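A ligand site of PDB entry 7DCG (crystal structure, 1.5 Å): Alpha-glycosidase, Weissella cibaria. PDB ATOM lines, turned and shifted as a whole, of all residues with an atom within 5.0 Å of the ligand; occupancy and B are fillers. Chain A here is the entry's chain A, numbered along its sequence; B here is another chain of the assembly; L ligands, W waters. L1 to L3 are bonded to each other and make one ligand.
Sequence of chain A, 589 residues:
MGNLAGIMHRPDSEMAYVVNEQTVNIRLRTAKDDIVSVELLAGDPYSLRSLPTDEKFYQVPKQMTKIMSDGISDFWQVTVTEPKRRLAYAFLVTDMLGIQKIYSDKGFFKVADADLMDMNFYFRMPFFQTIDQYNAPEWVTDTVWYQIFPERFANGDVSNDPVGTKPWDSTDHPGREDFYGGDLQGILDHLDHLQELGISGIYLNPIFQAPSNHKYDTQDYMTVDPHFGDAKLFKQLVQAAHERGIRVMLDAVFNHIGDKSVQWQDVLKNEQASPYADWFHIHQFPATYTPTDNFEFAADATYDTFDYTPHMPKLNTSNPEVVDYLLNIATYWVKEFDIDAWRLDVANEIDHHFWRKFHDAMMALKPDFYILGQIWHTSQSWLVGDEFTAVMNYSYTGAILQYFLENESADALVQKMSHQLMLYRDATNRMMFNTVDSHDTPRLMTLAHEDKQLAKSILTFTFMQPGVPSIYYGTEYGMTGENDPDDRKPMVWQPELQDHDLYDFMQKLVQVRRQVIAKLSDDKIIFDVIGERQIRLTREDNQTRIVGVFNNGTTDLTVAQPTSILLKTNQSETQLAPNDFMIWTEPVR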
ATOM      1  N   ARG A 176     -15.328  14.537  28.546  1.00  0.00           N
ATOM      2  CA  ARG A 176     -14.207  14.860  27.659  1.00  0.00           C
ATOM      3  C   ARG A 176     -13.514  16.156  28.032  1.00  0.00           C
ATOM      4  O   ARG A 176     -12.308  16.294  27.786  1.00  0.00           O
ATOM      5  CB  ARG A 176     -14.656  14.961  26.198  1.00  0.00           C
ATOM      6  CG  ARG A 176     -14.841  13.622  25.635  1.00  0.00           C
ATOM      7  CD  ARG A 176     -14.977  13.650  24.115  1.00  0.00           C
ATOM      8  NE  ARG A 176     -15.080  12.271  23.699  1.00  0.00           N
ATOM      9  CZ  ARG A 176     -14.077  11.514  23.207  1.00  0.00           C
ATOM     10  NH1 ARG A 176     -12.842  12.002  22.982  1.00  0.00           N
ATOM     11  NH2 ARG A 176     -14.356  10.249  22.875  1.00  0.00           N
ATOM     12  N   HIS A 214      -5.793  16.935  28.006  1.00  0.00           N
ATOM     13  CA  HIS A 214      -4.839  15.952  27.553  1.00  0.00           C
ATOM     14  C   HIS A 214      -3.595  16.562  26.906  1.00  0.00           C
ATOM     15  O   HIS A 214      -2.524  15.931  26.920  1.00  0.00           O
ATOM     16  CB  HIS A 214      -5.518  15.021  26.514  1.00  0.00           C
ATOM     17  CG  HIS A 214      -6.172  15.756  25.382  1.00  0.00           C
ATOM     18  ND1 HIS A 214      -5.460  16.240  24.293  1.00  0.00           N
ATOM     19  CD2 HIS A 214      -7.473  16.087  25.163  1.00  0.00           C
ATOM     20  CE1 HIS A 214      -6.300  16.831  23.456  1.00  0.00           C
ATOM     21  NE2 HIS A 214      -7.531  16.765  23.970  1.00  0.00           N
ATOM     22  N   TYR A 216      -2.671  17.322  23.868  1.00  0.00           N
ATOM     23  CA  TYR A 216      -2.132  16.967  22.533  1.00  0.00           C
ATOM     24  C   TYR A 216      -2.363  18.053  21.498  1.00  0.00           C
ATOM     25  O   TYR A 216      -1.912  17.889  20.360  1.00  0.00           O
ATOM     26  CB  TYR A 216      -2.753  15.619  22.057  1.00  0.00           C
ATOM     27  CG  TYR A 216      -2.124  14.441  22.753  1.00  0.00           C
ATOM     28  CD1 TYR A 216      -0.918  13.874  22.295  1.00  0.00           C
ATOM     29  CD2 TYR A 216      -2.693  13.906  23.906  1.00  0.00           C
ATOM     30  CE1 TYR A 216      -0.323  12.808  22.925  1.00  0.00           C
ATOM     31  CE2 TYR A 216      -2.084  12.815  24.579  1.00  0.00           C
ATOM     32  CZ  TYR A 216      -0.890  12.261  24.052  1.00  0.00           C
ATOM     33  OH  TYR A 216      -0.289  11.207  24.685  1.00  0.00           O
ATOM     34  N   VAL A 253       4.761  15.699  20.657  1.00  0.00           N
ATOM     35  CA  VAL A 253       3.590  15.708  19.808  1.00  0.00           C
ATOM     36  C   VAL A 253       3.958  16.511  18.570  1.00  0.00           C
ATOM     37  O   VAL A 253       3.622  17.694  18.473  1.00  0.00           O
ATOM     38  CB  VAL A 253       2.389  16.317  20.565  1.00  0.00           C
ATOM     39  CG1 VAL A 253       1.076  16.136  19.724  1.00  0.00           C
ATOM     40  CG2 VAL A 253       2.210  15.602  21.903  1.00  0.00           C
ATOM     41  N   HIS A 256       1.308  17.247  14.629  1.00  0.00           N
ATOM     42  CA  HIS A 256       0.318  18.302  14.476  1.00  0.00           C
ATOM     43  C   HIS A 256       0.528  19.243  15.652  1.00  0.00           C
ATOM     44  O   HIS A 256       1.130  18.880  16.666  1.00  0.00           O
ATOM     45  CB  HIS A 256      -1.122  17.738  14.478  1.00  0.00           C
ATOM     46  CG  HIS A 256      -1.353  16.720  15.557  1.00  0.00           C
ATOM     47  ND1 HIS A 256      -1.195  15.347  15.344  1.00  0.00           N
ATOM     48  CD2 HIS A 256      -1.683  16.877  16.861  1.00  0.00           C
ATOM     49  CE1 HIS A 256      -1.436  14.705  16.483  1.00  0.00           C
ATOM     50  NE2 HIS A 256      -1.723  15.611  17.421  1.00  0.00           N
ATOM     51  N   GLU A 296     -14.466  17.637  17.937  1.00  0.00           N
ATOM     52  CA  GLU A 296     -13.297  16.968  17.373  1.00  0.00           C
ATOM     53  C   GLU A 296     -13.504  16.478  15.955  1.00  0.00           C
ATOM     54  O   GLU A 296     -12.718  15.674  15.459  1.00  0.00           O
ATOM     55  CB  GLU A 296     -12.844  15.823  18.296  1.00  0.00           C
ATOM     56  CG  GLU A 296     -12.318  16.458  19.629  1.00  0.00           C
ATOM     57  CD  GLU A 296     -11.840  15.473  20.686  1.00  0.00           C
ATOM     58  OE1 GLU A 296     -12.383  14.375  20.748  1.00  0.00           O
ATOM     59  OE2 GLU A 296     -10.927  15.790  21.491  1.00  0.00           O
ATOM     60  N   PHE A 306      -4.656  16.008  12.091  1.00  0.00           N
ATOM     61  CA  PHE A 306      -4.776  14.718  12.756  1.00  0.00           C
ATOM     62  C   PHE A 306      -6.221  14.232  12.562  1.00  0.00           C
ATOM     63  O   PHE A 306      -7.156  15.015  12.755  1.00  0.00           O
ATOM     64  CB  PHE A 306      -4.458  14.814  14.260  1.00  0.00           C
ATOM     65  CG  PHE A 306      -4.677  13.503  14.941  1.00  0.00           C
ATOM     66  CD1 PHE A 306      -3.827  12.411  14.628  1.00  0.00           C
ATOM     67  CD2 PHE A 306      -5.769  13.296  15.789  1.00  0.00           C
ATOM     68  CE1 PHE A 306      -4.104  11.112  15.168  1.00  0.00           C
ATOM     69  CE2 PHE A 306      -6.048  12.011  16.338  1.00  0.00           C
ATOM     70  CZ  PHE A 306      -5.170  10.925  16.010  1.00  0.00           C
ATOM     71  N   THR A 309      -9.945  16.134  13.039  1.00  0.00           N
ATOM     72  CA  THR A 309     -10.205  17.237  13.971  1.00  0.00           C
ATOM     73  C   THR A 309      -9.632  18.564  13.457  1.00  0.00           C
ATOM     74  O   THR A 309      -8.415  18.654  13.225  1.00  0.00           O
ATOM     75  CB  THR A 309      -9.671  16.990  15.362  1.00  0.00           C
ATOM     76  OG1 THR A 309      -9.821  18.239  16.116  1.00  0.00           O
ATOM     77  CG2 THR A 309      -8.259  16.431  15.394  1.00  0.00           C
ATOM     78  N   MET A 312      -6.344  20.313  15.245  1.00  0.00           N
ATOM     79  CA  MET A 312      -4.968  19.787  15.207  1.00  0.00           C
ATOM     80  C   MET A 312      -4.433  19.816  13.775  1.00  0.00           C
ATOM     81  O   MET A 312      -4.288  18.764  13.122  1.00  0.00           O
ATOM     82  CB  MET A 312      -4.934  18.375  15.796  1.00  0.00           C
ATOM     83  CG  MET A 312      -5.243  18.347  17.275  1.00  0.00           C
ATOM     84  SD  MET A 312      -5.263  16.625  17.864  1.00  0.00           S
ATOM     85  CE  MET A 312      -5.462  16.936  19.629  1.00  0.00           C
ATOM     86  N   ARG A 343       8.813   9.800  23.871  1.00  0.00           N
ATOM     87  CA  ARG A 343       7.750   9.014  23.265  1.00  0.00           C
ATOM     88  C   ARG A 343       7.127   9.871  22.160  1.00  0.00           C
ATOM     89  O   ARG A 343       6.758  11.024  22.421  1.00  0.00           O
ATOM     90  CB  ARG A 343       6.702   8.668  24.315  1.00  0.00           C
ATOM     91  CG  ARG A 343       5.505   7.811  23.814  1.00  0.00           C
ATOM     92  CD  ARG A 343       4.358   8.751  23.367  1.00  0.00           C
ATOM     93  NE  ARG A 343       3.103   8.043  23.291  1.00  0.00           N
ATOM     94  CZ  ARG A 343       1.973   8.514  22.794  1.00  0.00           C
ATOM     95  NH1 ARG A 343       1.937   9.752  22.232  1.00  0.00           N
ATOM     96  NH2 ARG A 343       0.879   7.705  22.789  1.00  0.00           N
ATOM     97  N   ASP A 345       4.424  10.823  19.596  1.00  0.00           N
ATOM     98  CA  ASP A 345       3.000  10.685  19.269  1.00  0.00           C
ATOM     99  C   ASP A 345       2.754  10.592  17.739  1.00  0.00           C
ATOM    100  O   ASP A 345       3.317  11.358  16.964  1.00  0.00           O
ATOM    101  CB  ASP A 345       2.320  11.915  19.852  1.00  0.00           C
ATOM    102  CG  ASP A 345       0.822  11.889  19.718  1.00  0.00           C
ATOM    103  OD1 ASP A 345       0.220  10.927  20.273  1.00  0.00           O
ATOM    104  OD2 ASP A 345       0.239  12.815  19.088  1.00  0.00           O
ATOM    105  N   VAL A 346       1.886   9.665  17.309  1.00  0.00           N
ATOM    106  CA  VAL A 346       1.505   9.501  15.883  1.00  0.00           C
ATOM    107  C   VAL A 346       2.781   9.457  15.011  1.00  0.00           C
ATOM    108  O   VAL A 346       2.888  10.119  13.961  1.00  0.00           O
ATOM    109  CB  VAL A 346       0.494  10.569  15.360  1.00  0.00           C
ATOM    110  CG1 VAL A 346      -0.224   9.983  14.115  1.00  0.00           C
ATOM    111  CG2 VAL A 346      -0.542  10.974  16.427  1.00  0.00           C
ATOM    112  N   ASN A 348       4.303   7.457  13.080  1.00  0.00           N
ATOM    113  CA  ASN A 348       4.296   6.921  11.728  1.00  0.00           C
ATOM    114  C   ASN A 348       3.892   7.958  10.678  1.00  0.00           C
ATOM    115  O   ASN A 348       4.193   7.747   9.503  1.00  0.00           O
ATOM    116  CB  ASN A 348       3.349   5.715  11.645  1.00  0.00           C
ATOM    117  CG  ASN A 348       1.932   6.033  12.163  1.00  0.00           C
ATOM    118  OD1 ASN A 348       1.704   6.998  12.926  1.00  0.00           O
ATOM    119  ND2 ASN A 348       0.957   5.207  11.728  1.00  0.00           N
ATOM    120  N   GLU A 349       3.224   9.044  11.053  1.00  0.00           N
ATOM    121  CA  GLU A 349       2.719   9.975  10.049  1.00  0.00           C
ATOM    122  C   GLU A 349       3.716  11.111   9.765  1.00  0.00           C
ATOM    123  O   GLU A 349       3.410  12.018   8.979  1.00  0.00           O
ATOM    124  CB  GLU A 349       1.323  10.530  10.506  1.00  0.00           C
ATOM    125  CG  GLU A 349       0.350   9.343  10.496  1.00  0.00           C
ATOM    126  CD  GLU A 349      -1.091   9.670  10.886  1.00  0.00           C
ATOM    127  OE1 GLU A 349      -1.511  10.864  10.925  1.00  0.00           O
ATOM    128  OE2 GLU A 349      -1.851   8.700  11.170  1.00  0.00           O
ATOM    129  N   GLN A 374       5.106   5.900  18.841  1.00  0.00           N
ATOM    130  CA  GLN A 374       3.734   5.383  18.991  1.00  0.00           C
ATOM    131  C   GLN A 374       3.222   4.968  17.610  1.00  0.00           C
ATOM    132  O   GLN A 374       2.821   5.819  16.810  1.00  0.00           O
ATOM    133  CB  GLN A 374       2.798   6.395  19.633  1.00  0.00           C
ATOM    134  CG  GLN A 374       1.451   5.742  19.944  1.00  0.00           C
ATOM    135  CD  GLN A 374       0.292   6.678  19.791  1.00  0.00           C
ATOM    136  OE1 GLN A 374       0.407   7.749  19.151  1.00  0.00           O
ATOM    137  NE2 GLN A 374      -0.838   6.276  20.373  1.00  0.00           N
ATOM    138  N   TRP A 376       0.780   1.630  15.847  1.00  0.00           N
ATOM    139  CA  TRP A 376      -0.060   0.475  16.167  1.00  0.00           C
ATOM    140  C   TRP A 376       0.147  -0.680  15.222  1.00  0.00           C
ATOM    141  O   TRP A 376      -0.206  -1.810  15.560  1.00  0.00           O
ATOM    142  CB  TRP A 376      -1.543   0.865  16.109  1.00  0.00           C
ATOM    143  CG  TRP A 376      -2.043   1.655  17.235  1.00  0.00           C
ATOM    144  CD1 TRP A 376      -1.837   2.990  17.485  1.00  0.00           C
ATOM    145  CD2 TRP A 376      -2.865   1.155  18.276  1.00  0.00           C
ATOM    146  NE1 TRP A 376      -2.517   3.338  18.649  1.00  0.00           N
ATOM    147  CE2 TRP A 376      -3.155   2.224  19.136  1.00  0.00           C
ATOM    148  CE3 TRP A 376      -3.389  -0.116  18.539  1.00  0.00           C
ATOM    149  CZ2 TRP A 376      -3.964   2.045  20.287  1.00  0.00           C
ATOM    150  CZ3 TRP A 376      -4.168  -0.291  19.644  1.00  0.00           C
ATOM    151  CH2 TRP A 376      -4.445   0.784  20.517  1.00  0.00           C
ATOM    152  N   HIS A 439      -4.046   5.634  28.143  1.00  0.00           N
ATOM    153  CA  HIS A 439      -5.011   6.720  28.156  1.00  0.00           C
ATOM    154  C   HIS A 439      -5.900   6.695  26.917  1.00  0.00           C
ATOM    155  O   HIS A 439      -6.751   7.592  26.781  1.00  0.00           O
ATOM    156  CB  HIS A 439      -4.237   8.049  28.243  1.00  0.00           C
ATOM    157  CG  HIS A 439      -3.353   8.299  27.044  1.00  0.00           C
ATOM    158  ND1 HIS A 439      -2.314   7.440  26.714  1.00  0.00           N
ATOM    159  CD2 HIS A 439      -3.405   9.237  26.071  1.00  0.00           C
ATOM    160  CE1 HIS A 439      -1.745   7.862  25.603  1.00  0.00           C
ATOM    161  NE2 HIS A 439      -2.380   8.965  25.186  1.00  0.00           N
ATOM    162  N   ASP A 440      -5.681   5.765  25.984  1.00  0.00           N
ATOM    163  CA  ASP A 440      -6.521   5.629  24.782  1.00  0.00           C
ATOM    164  C   ASP A 440      -7.296   4.331  24.667  1.00  0.00           C
ATOM    165  O   ASP A 440      -7.853   4.055  23.585  1.00  0.00           O
ATOM    166  CB  ASP A 440      -5.698   5.691  23.513  1.00  0.00           C
ATOM    167  CG  ASP A 440      -4.947   6.923  23.332  1.00  0.00           C
ATOM    168  OD1 ASP A 440      -5.498   8.037  23.580  1.00  0.00           O
ATOM    169  OD2 ASP A 440      -3.775   6.782  22.903  1.00  0.00           O
ATOM    170  N   ASP A 484     -11.334   6.204  26.569  1.00  0.00           N
ATOM    171  CA  ASP A 484     -11.222   7.644  26.650  1.00  0.00           C
ATOM    172  C   ASP A 484     -12.583   8.300  26.432  1.00  0.00           C
ATOM    173  O   ASP A 484     -13.208   8.058  25.385  1.00  0.00           O
ATOM    174  CB  ASP A 484     -10.201   8.079  25.582  1.00  0.00           C
ATOM    175  CG  ASP A 484     -10.164   9.584  25.320  1.00  0.00           C
ATOM    176  OD1 ASP A 484     -10.568  10.365  26.211  1.00  0.00           O
ATOM    177  OD2 ASP A 484      -9.714   9.985  24.201  1.00  0.00           O
ATOM    178  N   ARG A 488      -9.504   7.813  32.136  1.00  0.00           N
ATOM    179  CA  ARG A 488      -8.719   8.929  32.686  1.00  0.00           C
ATOM    180  C   ARG A 488      -9.315   9.377  34.015  1.00  0.00           C
ATOM    181  O   ARG A 488      -9.350  10.568  34.347  1.00  0.00           O
ATOM    182  CB  ARG A 488      -8.649  10.069  31.659  1.00  0.00           C
ATOM    183  CG  ARG A 488      -7.912   9.670  30.420  1.00  0.00           C
ATOM    184  CD  ARG A 488      -8.279  10.565  29.241  1.00  0.00           C
ATOM    185  NE  ARG A 488      -7.613  10.078  28.012  1.00  0.00           N
ATOM    186  CZ  ARG A 488      -7.432  10.820  26.909  1.00  0.00           C
ATOM    187  NH1 ARG A 488      -7.773  12.129  26.874  1.00  0.00           N
ATOM    188  NH2 ARG A 488      -6.812  10.267  25.860  1.00  0.00           N
ATOM    189  N   TYR B  46      -8.629   6.608   8.940  1.00  0.00           N
ATOM    190  CA  TYR B  46      -9.477   7.319   9.880  1.00  0.00           C
ATOM    191  C   TYR B  46     -10.912   7.424   9.386  1.00  0.00           C
ATOM    192  O   TYR B  46     -11.829   7.737  10.177  1.00  0.00           O
ATOM    193  CB  TYR B  46      -8.914   8.724  10.119  1.00  0.00           C
ATOM    194  CG  TYR B  46      -7.593   8.689  10.838  1.00  0.00           C
ATOM    195  CD1 TYR B  46      -7.536   8.647  12.235  1.00  0.00           C
ATOM    196  CD2 TYR B  46      -6.388   8.653  10.119  1.00  0.00           C
ATOM    197  CE1 TYR B  46      -6.323   8.650  12.905  1.00  0.00           C
ATOM    198  CE2 TYR B  46      -5.179   8.623  10.764  1.00  0.00           C
ATOM    199  CZ  TYR B  46      -5.147   8.630  12.177  1.00  0.00           C
ATOM    200  OH  TYR B  46      -3.926   8.634  12.824  1.00  0.00           O
ATOM    201  N   MET B 119      -9.074   0.362  12.037  1.00  0.00           N
ATOM    202  CA  MET B 119      -7.983   0.785  11.158  1.00  0.00           C
ATOM    203  C   MET B 119      -6.700   0.009  11.437  1.00  0.00           C
ATOM    204  O   MET B 119      -5.888  -0.164  10.531  1.00  0.00           O
ATOM    205  CB  MET B 119      -7.728   2.294  11.275  1.00  0.00           C
ATOM    206  CG  MET B 119      -7.412   2.740  12.681  1.00  0.00           C
ATOM    207  SD  MET B 119      -7.358   4.575  12.772  1.00  0.00           S
ATOM    208  CE  MET B 119      -5.786   4.759  12.357  1.00  0.00           C
ATOM    209  N   ASN B 120      -6.514  -0.505  12.662  1.00  0.00           N
ATOM    210  CA  ASN B 120      -5.246  -1.179  12.949  1.00  0.00           C
ATOM    211  C   ASN B 120      -5.192  -2.625  12.459  1.00  0.00           C
ATOM    212  O   ASN B 120      -4.139  -3.272  12.587  1.00  0.00           O
ATOM    213  CB  ASN B 120      -5.004  -1.123  14.472  1.00  0.00           C
ATOM    214  CG  ASN B 120      -4.892   0.307  14.929  1.00  0.00           C
ATOM    215  OD1 ASN B 120      -4.306   1.103  14.220  1.00  0.00           O
ATOM    216  ND2 ASN B 120      -5.500   0.662  16.049  1.00  0.00           N
HETATM  217  C1  LIG L   1      -4.497   6.478  15.944  1.00  0.00           C
HETATM  218  C2  LIG L   1      -3.132   7.174  15.979  1.00  0.00           C
HETATM  219  C3  LIG L   1      -2.599   7.298  17.395  1.00  0.00           C
HETATM  220  C4  LIG L   1      -3.604   8.236  18.125  1.00  0.00           C
HETATM  221  C5  LIG L   1      -4.907   7.418  18.179  1.00  0.00           C
HETATM  222  C6  LIG L   1      -6.030   7.986  19.029  1.00  0.00           C
HETATM  223  O1  LIG L   1      -4.352   5.195  16.541  1.00  0.00           O
HETATM  224  O2  LIG L   1      -2.214   6.359  15.243  1.00  0.00           O
HETATM  225  O3  LIG L   1      -1.381   8.045  17.265  1.00  0.00           O
HETATM  226  O4  LIG L   1      -3.250   8.425  19.461  1.00  0.00           O
HETATM  227  O5  LIG L   1      -5.366   7.219  16.832  1.00  0.00           O
HETATM  228  O6  LIG L   1      -6.500   9.220  18.490  1.00  0.00           O
HETATM  229  C1  LG2 L   2      -2.310   9.452  19.861  1.00  0.00           C
HETATM  230  C2  LG2 L   2      -2.388   9.717  21.354  1.00  0.00           C
HETATM  231  C3  LG2 L   2      -3.835  10.166  21.675  1.00  0.00           C
HETATM  232  C4  LG2 L   2      -3.992  11.543  21.045  1.00  0.00           C
HETATM  233  C5  LG2 L   2      -3.763  11.429  19.552  1.00  0.00           C
HETATM  234  C6  LG2 L   2      -3.599  12.795  18.881  1.00  0.00           C
HETATM  235  O1  LG2 L   2      -1.986   8.591  22.126  1.00  0.00           O
HETATM  236  O2  LG2 L   2      -4.062  10.294  23.100  1.00  0.00           O
HETATM  237  O3  LG2 L   2      -5.389  11.875  21.243  1.00  0.00           O
HETATM  238  O4  LG2 L   2      -2.572  10.673  19.290  1.00  0.00           O
HETATM  239  O5  LG2 L   2      -2.457  13.538  19.404  1.00  0.00           O
HETATM  240  C1  LG3 L   3      -5.648  13.173  21.797  1.00  0.00           C
HETATM  241  C2  LG3 L   3      -6.527  13.016  23.033  1.00  0.00           C
HETATM  242  C3  LG3 L   3      -7.850  12.392  22.731  1.00  0.00           C
HETATM  243  C4  LG3 L   3      -8.496  13.203  21.598  1.00  0.00           C
HETATM  244  C5  LG3 L   3      -7.569  13.372  20.383  1.00  0.00           C
HETATM  245  C6  LG3 L   3      -8.150  14.255  19.255  1.00  0.00           C
HETATM  246  O1  LG3 L   3      -5.807  12.193  23.954  1.00  0.00           O
HETATM  247  O2  LG3 L   3      -8.663  12.429  23.927  1.00  0.00           O
HETATM  248  O3  LG3 L   3      -9.664  12.486  21.162  1.00  0.00           O
HETATM  249  O4  LG3 L   3      -6.328  13.961  20.841  1.00  0.00           O
HETATM  250  O5  LG3 L   3      -8.586  15.526  19.846  1.00  0.00           O
HETATM  251  O   HOH W   1     -10.725  14.456  23.990  1.00  0.00           O
HETATM  252  O   HOH W   2      -8.960  18.052  18.725  1.00  0.00           O
HETATM  253  O   HOH W   3      -6.372   3.565  16.759  1.00  0.00           O
HETATM  254  O   HOH W   4      -3.151   3.601  14.232  1.00  0.00           O
HETATM  255  O   HOH W   5      -0.398   3.667  14.313  1.00  0.00           O
HETATM  256  O   HOH W   6       0.505   6.145  15.288  1.00  0.00           O
HETATM  257  O   HOH W   7      -8.671   9.874  20.104  1.00  0.00           O
HETATM  258  O   HOH W   8      -1.694   6.316  12.622  1.00  0.00           O
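The side-chain carboxylate (OD1) of Asp 345 sits close to the side-chain amide oxygen (OE1) of Gln 374 (3.4 Å). OD1 of Asp 440 is in salt-bridge range of NH2 of Arg 488 (3.4 Å). OD2 of Asp 484 is in salt-bridge range of NH2 of Arg 488, at 3.4 Å. NH1 of Arg 343 is in salt-bridge range of OD1 of Asp 345 (2.9 Å). The guanidinium group of Arg 488 is in hydrogen-bond range of the backbone carbonyl oxygen of His 439 (2.8 Å). The side-chain sulfur (SD) of Met 312 sits at hydrogen-bond distance from a ring nitrogen (NE2) of His 256 (3.7 Å). OH of Tyr 216 is in hydrogen-bond range of NE2 of His 439 (3.1 Å). O of Val 346 lies close to OD1 of Asn 348.
Water W3 bridges O1 of LIG L1 and ND2 of Asn 120 of chain B. Water W8 lies within hydrogen-bond range of an oxygen (O2) of LIG L1, the side-chain carboxylate (OE2) of Glu 349, the side-chain amide nitrogen (ND2) of Asn 348 and the side-chain hydroxyl (OH) of Tyr 46 of chain B. Water W6 lies within hydrogen-bond range of O2 of LIG L1, OD1 of Asn 348 and O of Gln 374. Water W2 bridges the side-chain hydroxyl (OG1) of Thr 309 and an oxygen (O5) of LG3 L3. Water W4 bridges the side-chain amide oxygen (OD1) of Asn 120 of chain B and an oxygen (O1) of LIG L1. Water W5 lies within hydrogen-bond range of the backbone NH of Trp 376 (2.8 Å), the side-chain amide nitrogen of Asn 348 (3.3 Å) and an oxygen (O2) of LIG L1 (3.4 Å).
OE1 of Gln 374 lies within hydrogen-bond range of O3 of LIG L1 (2.6 Å). O1 of LG2 L2 is in hydrogen-bond range of OD2 of Asp 440. An oxygen (O2) of LG3 L3 is in hydrogen-bond range of the side-chain carboxylate (OD2) of Asp 484, 2.7 Å away. An oxygen (O5) of LG2 L2 lies within hydrogen-bond range of the side-chain carboxylate of Asp 345, 2.8 Å away. OE2 of Glu 296 lies within hydrogen-bond range of O5 of LG3 L3 (2.9 Å). O1 of LG3 L3 is in hydrogen-bond range of NH2 of Arg 488, 2.9 Å away. O5 of LG2 L2 is in hydrogen-bond range of NE2 of His 256. O2 of LG2 L2 sits at hydrogen-bond distance from NE2 of His 439, at 3.0 Å. NH2 of Arg 343 is in hydrogen-bond range of O1 of LG2 L2 (3.1 Å). NE1 of Trp 376 sits at hydrogen-bond distance from O1 of LIG L1 (3.4 Å).
Merely in contact with the ligand: Arg 176, His 214, Tyr 216, Phe 306, Met 312, Val 346 and Tyr 46 of chain B. Hydrophobic or aromatic side chains within 4 Å of the ligand: His 214, Tyr 216, His 256, Phe 306, Met 312, Val 346, Trp 376 and His 439. Within 4 Å of the ligand: Arg 176, His 214, Tyr 216, His 256, Glu 296, Phe 306, Met 312, Arg 343, Asp 345, Val 346, Gln 374, Trp 376, His 439, Asp 440, Asp 484, Arg 488 and Tyr 46 of chain B. The nearest printed residue that does not touch the ligand is Met 119 of chain B (4.2 Å).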
